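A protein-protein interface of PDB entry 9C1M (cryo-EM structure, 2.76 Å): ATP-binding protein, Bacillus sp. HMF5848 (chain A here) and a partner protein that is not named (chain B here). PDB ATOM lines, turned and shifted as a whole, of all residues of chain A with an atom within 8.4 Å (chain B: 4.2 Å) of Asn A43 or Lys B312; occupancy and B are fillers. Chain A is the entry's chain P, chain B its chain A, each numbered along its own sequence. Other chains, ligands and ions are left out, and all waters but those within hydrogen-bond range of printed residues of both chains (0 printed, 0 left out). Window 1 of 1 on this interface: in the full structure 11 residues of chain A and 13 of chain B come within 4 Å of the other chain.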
ATOM      1  N   MET A   1     -12.052  25.981  10.166  1.00  0.00           N
ATOM      2  CA  MET A   1     -11.775  27.378  10.473  1.00  0.00           C
ATOM      3  C   MET A   1     -13.044  28.220  10.396  1.00  0.00           C
ATOM      4  O   MET A   1     -13.807  28.123   9.436  1.00  0.00           O
ATOM      5  CB  MET A   1     -10.715  27.938   9.521  1.00  0.00           C
ATOM      6  CG  MET A   1      -9.297  27.500   9.845  1.00  0.00           C
ATOM      7  SD  MET A   1      -8.990  25.775   9.423  1.00  0.00           S
ATOM      8  CE  MET A   1      -8.892  25.876   7.637  1.00  0.00           C
ATOM      9  N   GLN A  40      -9.000  25.525  19.108  1.00  0.00           N
ATOM     10  CA  GLN A  40      -9.072  24.077  19.222  1.00  0.00           C
ATOM     11  C   GLN A  40      -7.701  23.496  19.538  1.00  0.00           C
ATOM     12  O   GLN A  40      -6.678  23.952  19.019  1.00  0.00           O
ATOM     13  CB  GLN A  40      -9.612  23.466  17.929  1.00  0.00           C
ATOM     14  CG  GLN A  40     -10.122  22.044  18.090  1.00  0.00           C
ATOM     15  CD  GLN A  40     -10.922  21.565  16.897  1.00  0.00           C
ATOM     16  OE1 GLN A  40     -11.211  22.330  15.980  1.00  0.00           O
ATOM     17  NE2 GLN A  40     -11.287  20.289  16.905  1.00  0.00           N
ATOM     18  N   GLU A  41      -7.685  22.490  20.407  1.00  0.00           N
ATOM     19  CA  GLU A  41      -6.487  21.715  20.707  1.00  0.00           C
ATOM     20  C   GLU A  41      -6.894  20.250  20.701  1.00  0.00           C
ATOM     21  O   GLU A  41      -7.596  19.793  21.608  1.00  0.00           O
ATOM     22  CB  GLU A  41      -5.879  22.118  22.051  1.00  0.00           C
ATOM     23  CG  GLU A  41      -4.900  21.106  22.622  1.00  0.00           C
ATOM     24  CD  GLU A  41      -4.180  21.619  23.854  1.00  0.00           C
ATOM     25  OE1 GLU A  41      -4.064  22.854  24.004  1.00  0.00           O
ATOM     26  OE2 GLU A  41      -3.731  20.789  24.672  1.00  0.00           O
ATOM     27  N   GLY A  42      -6.471  19.518  19.677  1.00  0.00           N
ATOM     28  CA  GLY A  42      -6.935  18.162  19.491  1.00  0.00           C
ATOM     29  C   GLY A  42      -8.325  18.126  18.885  1.00  0.00           C
ATOM     30  O   GLY A  42      -8.923  19.145  18.540  1.00  0.00           O
ATOM     31  N   ASN A  43      -8.850  16.907  18.756  1.00  0.00           N
ATOM     32  CA  ASN A  43     -10.148  16.718  18.123  1.00  0.00           C
ATOM     33  C   ASN A  43     -11.318  17.068  19.034  1.00  0.00           C
ATOM     34  O   ASN A  43     -12.411  17.346  18.530  1.00  0.00           O
ATOM     35  CB  ASN A  43     -10.295  15.272  17.645  1.00  0.00           C
ATOM     36  CG  ASN A  43      -9.242  14.888  16.625  1.00  0.00           C
ATOM     37  OD1 ASN A  43      -8.725  15.736  15.900  1.00  0.00           O
ATOM     38  ND2 ASN A  43      -8.917  13.602  16.566  1.00  0.00           N
ATOM     39  N   HIS A  44     -11.122  17.070  20.354  1.00  0.00           N
ATOM     40  CA  HIS A  44     -12.230  17.228  21.287  1.00  0.00           C
ATOM     41  C   HIS A  44     -12.059  18.357  22.295  1.00  0.00           C
ATOM     42  O   HIS A  44     -13.033  18.693  22.977  1.00  0.00           O
ATOM     43  CB  HIS A  44     -12.463  15.922  22.062  1.00  0.00           C
ATOM     44  CG  HIS A  44     -12.920  14.784  21.204  1.00  0.00           C
ATOM     45  ND1 HIS A  44     -12.498  13.488  21.404  1.00  0.00           N
ATOM     46  CD2 HIS A  44     -13.758  14.748  20.141  1.00  0.00           C
ATOM     47  CE1 HIS A  44     -13.058  12.701  20.502  1.00  0.00           C
ATOM     48  NE2 HIS A  44     -13.827  13.441  19.724  1.00  0.00           N
ATOM     49  N   ASN A  45     -10.875  18.949  22.412  1.00  0.00           N
ATOM     50  CA  ASN A  45     -10.591  19.922  23.454  1.00  0.00           C
ATOM     51  C   ASN A  45     -10.472  21.322  22.863  1.00  0.00           C
ATOM     52  O   ASN A  45     -10.090  21.496  21.703  1.00  0.00           O
ATOM     53  CB  ASN A  45      -9.303  19.561  24.198  1.00  0.00           C
ATOM     54  CG  ASN A  45      -9.425  18.268  24.977  1.00  0.00           C
ATOM     55  OD1 ASN A  45     -10.499  17.671  25.048  1.00  0.00           O
ATOM     56  ND2 ASN A  45      -8.316  17.818  25.552  1.00  0.00           N
ATOM     57  N   PHE A  46     -10.806  22.318  23.680  1.00  0.00           N
ATOM     58  CA  PHE A  46     -10.743  23.718  23.287  1.00  0.00           C
ATOM     59  C   PHE A  46      -9.951  24.503  24.322  1.00  0.00           C
ATOM     60  O   PHE A  46      -9.948  24.167  25.508  1.00  0.00           O
ATOM     61  CB  PHE A  46     -12.142  24.330  23.142  1.00  0.00           C
ATOM     62  CG  PHE A  46     -12.907  23.829  21.953  1.00  0.00           C
ATOM     63  CD1 PHE A  46     -12.766  24.435  20.717  1.00  0.00           C
ATOM     64  CD2 PHE A  46     -13.774  22.758  22.072  1.00  0.00           C
ATOM     65  CE1 PHE A  46     -13.474  23.979  19.622  1.00  0.00           C
ATOM     66  CE2 PHE A  46     -14.483  22.296  20.982  1.00  0.00           C
ATOM     67  CZ  PHE A  46     -14.332  22.906  19.755  1.00  0.00           C
ATOM     68  N   PHE A  75     -11.013  23.234  27.804  1.00  0.00           N
ATOM     69  CA  PHE A  75     -12.309  22.558  27.804  1.00  0.00           C
ATOM     70  C   PHE A  75     -12.081  21.076  27.520  1.00  0.00           C
ATOM     71  O   PHE A  75     -12.014  20.656  26.362  1.00  0.00           O
ATOM     72  CB  PHE A  75     -13.260  23.180  26.783  1.00  0.00           C
ATOM     73  CG  PHE A  75     -14.195  24.194  27.369  1.00  0.00           C
ATOM     74  CD1 PHE A  75     -15.417  23.804  27.889  1.00  0.00           C
ATOM     75  CD2 PHE A  75     -13.855  25.535  27.404  1.00  0.00           C
ATOM     76  CE1 PHE A  75     -16.283  24.729  28.431  1.00  0.00           C
ATOM     77  CE2 PHE A  75     -14.718  26.465  27.946  1.00  0.00           C
ATOM     78  CZ  PHE A  75     -15.932  26.060  28.460  1.00  0.00           C
ATOM     79  N   SER A  89      -1.416  23.556  18.515  1.00  0.00           N
ATOM     80  CA  SER A  89      -0.553  23.390  17.357  1.00  0.00           C
ATOM     81  C   SER A  89      -0.820  24.484  16.322  1.00  0.00           C
ATOM     82  O   SER A  89      -1.903  25.071  16.287  1.00  0.00           O
ATOM     83  CB  SER A  89      -0.770  22.013  16.737  1.00  0.00           C
ATOM     84  OG  SER A  89       0.302  21.653  15.884  1.00  0.00           O
ATOM     85  N   PRO A  90       0.166  24.785  15.476  1.00  0.00           N
ATOM     86  CA  PRO A  90      -0.059  25.748  14.394  1.00  0.00           C
ATOM     87  C   PRO A  90      -1.127  25.266  13.425  1.00  0.00           C
ATOM     88  O   PRO A  90      -1.391  24.069  13.288  1.00  0.00           O
ATOM     89  CB  PRO A  90       1.309  25.834  13.711  1.00  0.00           C
ATOM     90  CG  PRO A  90       2.271  25.533  14.792  1.00  0.00           C
ATOM     91  CD  PRO A  90       1.599  24.500  15.662  1.00  0.00           C
ATOM     92  N   THR A  91      -1.746  26.232  12.745  1.00  0.00           N
ATOM     93  CA  THR A  91      -2.856  25.981  11.822  1.00  0.00           C
ATOM     94  C   THR A  91      -4.003  25.252  12.519  1.00  0.00           C
ATOM     95  O   THR A  91      -4.589  24.312  11.978  1.00  0.00           O
ATOM     96  CB  THR A  91      -2.396  25.212  10.578  1.00  0.00           C
ATOM     97  OG1 THR A  91      -2.076  23.861  10.931  1.00  0.00           O
ATOM     98  CG2 THR A  91      -1.173  25.875   9.961  1.00  0.00           C
ATOM     99  N   GLU A  92      -4.322  25.689  13.744  1.00  0.00           N
ATOM    100  CA  GLU A  92      -5.487  25.205  14.473  1.00  0.00           C
ATOM    101  C   GLU A  92      -6.584  26.257  14.439  1.00  0.00           C
ATOM    102  O   GLU A  92      -6.315  27.432  14.723  1.00  0.00           O
ATOM    103  CB  GLU A  92      -5.127  24.873  15.919  1.00  0.00           C
ATOM    104  CG  GLU A  92      -4.683  23.431  16.133  1.00  0.00           C
ATOM    105  CD  GLU A  92      -5.821  22.436  16.002  1.00  0.00           C
ATOM    106  OE1 GLU A  92      -6.167  22.071  14.859  1.00  0.00           O
ATOM    107  OE2 GLU A  92      -6.366  22.010  17.042  1.00  0.00           O
ATOM    108  N   PRO A  93      -7.808  25.882  14.089  1.00  0.00           N
ATOM    109  CA  PRO A  93      -8.863  26.884  13.887  1.00  0.00           C
ATOM    110  C   PRO A  93      -9.270  27.596  15.171  1.00  0.00           C
ATOM    111  O   PRO A  93      -9.118  27.077  16.279  1.00  0.00           O
ATOM    112  CB  PRO A  93     -10.026  26.060  13.323  1.00  0.00           C
ATOM    113  CG  PRO A  93      -9.676  24.631  13.617  1.00  0.00           C
ATOM    114  CD  PRO A  93      -8.207  24.539  13.638  1.00  0.00           C
ATOM    115  N   PHE A  95     -12.605  29.660  16.891  1.00  0.00           N
ATOM    116  CA  PHE A  95     -14.038  29.438  16.708  1.00  0.00           C
ATOM    117  C   PHE A  95     -14.964  30.475  17.341  1.00  0.00           C
ATOM    118  O   PHE A  95     -16.180  30.246  17.354  1.00  0.00           O
ATOM    119  CB  PHE A  95     -14.425  28.053  17.231  1.00  0.00           C
ATOM    120  CG  PHE A  95     -13.845  26.924  16.440  1.00  0.00           C
ATOM    121  CD1 PHE A  95     -14.436  26.527  15.254  1.00  0.00           C
ATOM    122  CD2 PHE A  95     -12.719  26.254  16.880  1.00  0.00           C
ATOM    123  CE1 PHE A  95     -13.916  25.487  14.520  1.00  0.00           C
ATOM    124  CE2 PHE A  95     -12.193  25.213  16.148  1.00  0.00           C
ATOM    125  CZ  PHE A  95     -12.797  24.827  14.967  1.00  0.00           C
ATOM    126  N   LEU B 275      -8.420   9.421  20.687  1.00  0.00           N
ATOM    127  CA  LEU B 275      -9.352  10.037  19.755  1.00  0.00           C
ATOM    128  C   LEU B 275      -9.226  11.552  19.738  1.00  0.00           C
ATOM    129  O   LEU B 275      -9.887  12.208  18.925  1.00  0.00           O
ATOM    130  CB  LEU B 275     -10.796   9.645  20.099  1.00  0.00           C
ATOM    131  CG  LEU B 275     -11.357   8.393  19.422  1.00  0.00           C
ATOM    132  CD1 LEU B 275     -12.832   8.219  19.747  1.00  0.00           C
ATOM    133  CD2 LEU B 275     -11.143   8.449  17.919  1.00  0.00           C
ATOM    134  N   ASN B 276      -8.403  12.114  20.621  1.00  0.00           N
ATOM    135  CA  ASN B 276      -8.118  13.539  20.670  1.00  0.00           C
ATOM    136  C   ASN B 276      -6.802  13.896  19.993  1.00  0.00           C
ATOM    137  O   ASN B 276      -6.434  15.074  19.964  1.00  0.00           O
ATOM    138  CB  ASN B 276      -8.101  14.014  22.128  1.00  0.00           C
ATOM    139  CG  ASN B 276      -8.232  15.516  22.257  1.00  0.00           C
ATOM    140  OD1 ASN B 276      -9.222  16.104  21.823  1.00  0.00           O
ATOM    141  ND2 ASN B 276      -7.231  16.148  22.857  1.00  0.00           N
ATOM    142  N   ILE B 277      -6.088  12.916  19.449  1.00  0.00           N
ATOM    143  CA  ILE B 277      -4.800  13.140  18.804  1.00  0.00           C
ATOM    144  C   ILE B 277      -5.030  13.282  17.306  1.00  0.00           C
ATOM    145  O   ILE B 277      -5.719  12.456  16.694  1.00  0.00           O
ATOM    146  CB  ILE B 277      -3.818  11.998  19.111  1.00  0.00           C
ATOM    147  CG1 ILE B 277      -3.920  11.576  20.578  1.00  0.00           C
ATOM    148  CG2 ILE B 277      -2.395  12.400  18.762  1.00  0.00           C
ATOM    149  CD1 ILE B 277      -3.037  10.400  20.935  1.00  0.00           C
ATOM    150  N   ASN B 278      -4.458  14.333  16.716  1.00  0.00           N
ATOM    151  CA  ASN B 278      -4.711  14.633  15.310  1.00  0.00           C
ATOM    152  C   ASN B 278      -4.111  13.572  14.393  1.00  0.00           C
ATOM    153  O   ASN B 278      -4.765  13.113  13.448  1.00  0.00           O
ATOM    154  CB  ASN B 278      -4.159  16.016  14.967  1.00  0.00           C
ATOM    155  CG  ASN B 278      -4.819  17.120  15.768  1.00  0.00           C
ATOM    156  OD1 ASN B 278      -4.170  17.798  16.564  1.00  0.00           O
ATOM    157  ND2 ASN B 278      -6.115  17.309  15.556  1.00  0.00           N
ATOM    158  N   ARG B 282      -6.224   5.118  12.292  1.00  0.00           N
ATOM    159  CA  ARG B 282      -7.348   4.345  12.803  1.00  0.00           C
ATOM    160  C   ARG B 282      -7.915   3.488  11.680  1.00  0.00           C
ATOM    161  O   ARG B 282      -8.312   4.012  10.632  1.00  0.00           O
ATOM    162  CB  ARG B 282      -8.426   5.261  13.381  1.00  0.00           C
ATOM    163  CG  ARG B 282      -7.885   6.358  14.286  1.00  0.00           C
ATOM    164  CD  ARG B 282      -9.010   7.198  14.868  1.00  0.00           C
ATOM    165  NE  ARG B 282      -8.522   8.170  15.839  1.00  0.00           N
ATOM    166  CZ  ARG B 282      -8.062   9.374  15.528  1.00  0.00           C
ATOM    167  NH1 ARG B 282      -8.016   9.795  14.275  1.00  0.00           N
ATOM    168  NH2 ARG B 282      -7.639  10.177  16.500  1.00  0.00           N
ATOM    169  N   LYS B 308     -14.714  15.503  11.133  1.00  0.00           N
ATOM    170  CA  LYS B 308     -14.255  15.657  12.508  1.00  0.00           C
ATOM    171  C   LYS B 308     -12.836  15.161  12.730  1.00  0.00           C
ATOM    172  O   LYS B 308     -12.079  15.792  13.472  1.00  0.00           O
ATOM    173  CB  LYS B 308     -15.201  14.923  13.471  1.00  0.00           C
ATOM    174  CG  LYS B 308     -14.949  15.244  14.934  1.00  0.00           C
ATOM    175  CD  LYS B 308     -16.077  14.745  15.820  1.00  0.00           C
ATOM    176  CE  LYS B 308     -15.769  14.998  17.285  1.00  0.00           C
ATOM    177  NZ  LYS B 308     -15.349  16.405  17.528  1.00  0.00           N
ATOM    178  N   TYR B 309     -12.451  14.046  12.108  1.00  0.00           N
ATOM    179  CA  TYR B 309     -11.132  13.464  12.305  1.00  0.00           C
ATOM    180  C   TYR B 309     -10.222  13.568  11.089  1.00  0.00           C
ATOM    181  O   TYR B 309      -9.031  13.254  11.205  1.00  0.00           O
ATOM    182  CB  TYR B 309     -11.255  11.987  12.708  1.00  0.00           C
ATOM    183  CG  TYR B 309     -11.988  11.757  14.010  1.00  0.00           C
ATOM    184  CD1 TYR B 309     -11.330  11.853  15.225  1.00  0.00           C
ATOM    185  CD2 TYR B 309     -13.337  11.437  14.023  1.00  0.00           C
ATOM    186  CE1 TYR B 309     -11.994  11.642  16.417  1.00  0.00           C
ATOM    187  CE2 TYR B 309     -14.009  11.224  15.212  1.00  0.00           C
ATOM    188  CZ  TYR B 309     -13.333  11.328  16.405  1.00  0.00           C
ATOM    189  OH  TYR B 309     -13.996  11.117  17.591  1.00  0.00           O
ATOM    190  N   ASN B 310     -10.736  13.987   9.935  1.00  0.00           N
ATOM    191  CA  ASN B 310      -9.935  14.085   8.719  1.00  0.00           C
ATOM    192  C   ASN B 310     -10.245  15.379   7.981  1.00  0.00           C
ATOM    193  O   ASN B 310     -10.409  15.394   6.756  1.00  0.00           O
ATOM    194  CB  ASN B 310     -10.162  12.877   7.812  1.00  0.00           C
ATOM    195  CG  ASN B 310      -9.021  12.654   6.841  1.00  0.00           C
ATOM    196  OD1 ASN B 310      -8.025  13.375   6.859  1.00  0.00           O
ATOM    197  ND2 ASN B 310      -9.163  11.651   5.982  1.00  0.00           N
ATOM    198  N   SER B 311     -10.332  16.486   8.717  1.00  0.00           N
ATOM    199  CA  SER B 311     -10.686  17.777   8.138  1.00  0.00           C
ATOM    200  C   SER B 311      -9.494  18.712   7.980  1.00  0.00           C
ATOM    201  O   SER B 311      -9.367  19.369   6.943  1.00  0.00           O
ATOM    202  CB  SER B 311     -11.757  18.461   8.992  1.00  0.00           C
ATOM    203  OG  SER B 311     -11.252  18.798  10.272  1.00  0.00           O
ATOM    204  N   LYS B 312      -8.624  18.796   8.983  1.00  0.00           N
ATOM    205  CA  LYS B 312      -7.463  19.671   8.894  1.00  0.00           C
ATOM    206  C   LYS B 312      -6.487  19.148   7.848  1.00  0.00           C
ATOM    207  O   LYS B 312      -6.192  17.949   7.798  1.00  0.00           O
ATOM    208  CB  LYS B 312      -6.780  19.784  10.255  1.00  0.00           C
ATOM    209  CG  LYS B 312      -7.663  20.380  11.341  1.00  0.00           C
ATOM    210  CD  LYS B 312      -7.443  19.694  12.679  1.00  0.00           C
ATOM    211  CE  LYS B 312      -8.502  20.102  13.689  1.00  0.00           C
ATOM    212  NZ  LYS B 312      -8.199  19.589  15.052  1.00  0.00           N
ATOM    213  N   ILE B 313      -5.980  20.056   7.010  1.00  0.00           N
ATOM    214  CA  ILE B 313      -5.112  19.664   5.900  1.00  0.00           C
ATOM    215  C   ILE B 313      -3.655  19.529   6.304  1.00  0.00           C
ATOM    216  O   ILE B 313      -2.860  18.965   5.540  1.00  0.00           O
ATOM    217  CB  ILE B 313      -5.244  20.672   4.741  1.00  0.00           C
ATOM    218  CG1 ILE B 313      -4.896  20.010   3.407  1.00  0.00           C
ATOM    219  CG2 ILE B 313      -4.370  21.892   4.985  1.00  0.00           C
ATOM    220  CD1 ILE B 313      -6.011  19.164   2.835  1.00  0.00           C
ATOM    221  N   LYS B 314      -3.276  20.019   7.485  1.00  0.00           N
ATOM    222  CA  LYS B 314      -1.897  19.946   7.944  1.00  0.00           C
ATOM    223  C   LYS B 314      -1.721  19.135   9.221  1.00  0.00           C
ATOM    224  O   LYS B 314      -0.620  18.626   9.458  1.00  0.00           O
ATOM    225  CB  LYS B 314      -1.332  21.363   8.157  1.00  0.00           C
ATOM    226  CG  LYS B 314       0.128  21.426   8.584  1.00  0.00           C
ATOM    227  CD  LYS B 314       0.622  22.863   8.658  1.00  0.00           C
ATOM    228  CE  LYS B 314       2.031  22.936   9.225  1.00  0.00           C
ATOM    229  NZ  LYS B 314       3.027  22.297   8.323  1.00  0.00           N
ATOM    230  N   LEU B 315      -2.768  18.975  10.028  1.00  0.00           N
ATOM    231  CA  LEU B 315      -2.694  18.209  11.266  1.00  0.00           C
ATOM    232  C   LEU B 315      -3.227  16.790  11.124  1.00  0.00           C
ATOM    233  O   LEU B 315      -2.650  15.859  11.693  1.00  0.00           O
ATOM    234  CB  LEU B 315      -3.462  18.930  12.378  1.00  0.00           C
ATOM    235  CG  LEU B 315      -2.633  19.846  13.280  1.00  0.00           C
ATOM    236  CD1 LEU B 315      -2.104  21.031  12.501  1.00  0.00           C
ATOM    237  CD2 LEU B 315      -3.452  20.309  14.471  1.00  0.00           C
ATOM    238  N   HIS B 316      -4.318  16.601  10.380  1.00  0.00           N
ATOM    239  CA  HIS B 316      -4.896  15.274  10.167  1.00  0.00           C
ATOM    240  C   HIS B 316      -4.220  14.658   8.944  1.00  0.00           C
ATOM    241  O   HIS B 316      -4.708  14.730   7.814  1.00  0.00           O
ATOM    242  CB  HIS B 316      -6.406  15.372   9.997  1.00  0.00           C
ATOM    243  CG  HIS B 316      -7.138  15.660  11.272  1.00  0.00           C
ATOM    244  ND1 HIS B 316      -8.377  16.265  11.298  1.00  0.00           N
ATOM    245  CD2 HIS B 316      -6.804  15.432  12.563  1.00  0.00           C
ATOM    246  CE1 HIS B 316      -8.775  16.394  12.550  1.00  0.00           C
ATOM    247  NE2 HIS B 316      -7.839  15.897  13.338  1.00  0.00           N
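NH2 of Arg B282 sits at hydrogen-bond distance from O of Ile B277 (3.0 Å). The side-chain amide nitrogen of Asn B278 lies within hydrogen-bond range of a ring nitrogen (NE2) of His B316. A ring nitrogen (ND1) of His B316 lies close to the backbone carbonyl oxygen (O) of Tyr B309 (3.1 Å). N of Ser B311 sits at hydrogen-bond distance from ND1 of His B316 (3.2 Å). The backbone NH (N) of Lys B312 sits at hydrogen-bond distance from a ring nitrogen (ND1) of His B316, at 3.4 Å. NE2 of Gln A40 sits at hydrogen-bond distance from O of Gly A42, at 3.1 Å.
Of the 15 printed residues of chain A, 10 touch a printed residue of chain B. Of the 14 printed residues of chain B, 11 touch a printed residue of chain A. Printed residues of chain B that touch a printed residue of chain A: Leu B275, Asn B276, Ile B277, Asn B278, Arg B282, Lys B308, Tyr B309, Lys B312, Lys B314, Leu B315 and His B316. Hydrophobic or aromatic side chains of chain B within 4 Å of the printed part of chain A: Leu B275, Tyr B309, Leu B315 and His B316. Among the printed residues, 24 pairs touch across the chains.
O of Leu B275 is in hydrogen-bond range of ND2 of Asn A43 (2.9 Å). The side-chain amide oxygen of Asn B276 is in hydrogen-bond range of the backbone NH of Asn A43. N of His A44 lies within hydrogen-bond range of OD1 of Asn B276 (2.6 Å). The backbone NH (N) of Asn A45 is in hydrogen-bond range of the side-chain amide oxygen (OD1) of Asn B276 (3.3 Å). The backbone carbonyl oxygen (O) of Ile B277 is in hydrogen-bond range of the side-chain amide nitrogen (ND2) of Asn A43 (3.4 Å). The side-chain amide nitrogen (ND2) of Asn B278 is in hydrogen-bond range of the side-chain amide oxygen (OD1) of Asn A43, 3.1 Å away. The backbone carbonyl oxygen (O) of Asn A43 sits at hydrogen-bond distance from the side-chain amino group (NZ) of Lys B308 (3.2 Å). The side-chain hydroxyl (OH) of Tyr B309 is in hydrogen-bond range of a ring nitrogen (NE2) of His A44, 3.2 Å away. The side-chain carboxylate (OE1) of Glu A92 lies within salt-bridge range of the side-chain amino group (NZ) of Lys B312, at 3.2 Å. A ring nitrogen (NE2) of His B316 sits at hydrogen-bond distance from the side-chain amide oxygen (OD1) of Asn A43 (2.7 Å).
NE2 of Gln A40 touches NZ of Lys B312, 3.7 Å away. Glu A41 touches Asn B276. O of Asn B276 touches CA of Gly A42 (3.2 Å). O of Gly A42 touches NZ of Lys B312, at 3.6 Å. Asn A43 touches Tyr B309. Asn A43 touches Lys B312 (OD1 to NZ, 3.98 Å). NZ of Lys B308 touches CD2 of His A44, at 3.5 Å. Leu B315 touches Ser A89. Pro A90 touches Leu B315. Leu B315 touches Thr A91.
Of the printed residues of chain B, Asn A43 touches Leu B275 (2.9 Å), Asn B276 (3.2 Å), Ile B277 (3.4 Å), Asn B278 (3.1 Å), Arg B282 (3.7 Å), Lys B308 (3.2 Å), Tyr B309 (3.3 Å), Lys B312 (3.98 Å) and His B316 (2.7 Å). Of the printed residues of chain A, Lys B312 touches Gln A40 (3.7 Å), Gly A42 (3.6 Å), Asn A43 (3.98 Å) and Glu A92 (3.2 Å). Printed residues of chain A within 4 Å of Ile B277: Asn A43. Of the printed residues of chain A, Asn B278 touches Asn A43 (3.1 Å). Of the printed residues of chain A, Tyr B309 touches Asn A43 and His A44. Pro A93 touches none of the printed residues of chain B. The nearest printed residue of chain B that does not touch Asn A43 is Asn B310 (6.5 Å). The nearest printed residue of chain A that does not touch Lys B312 is Pro A93 (4.4 Å).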
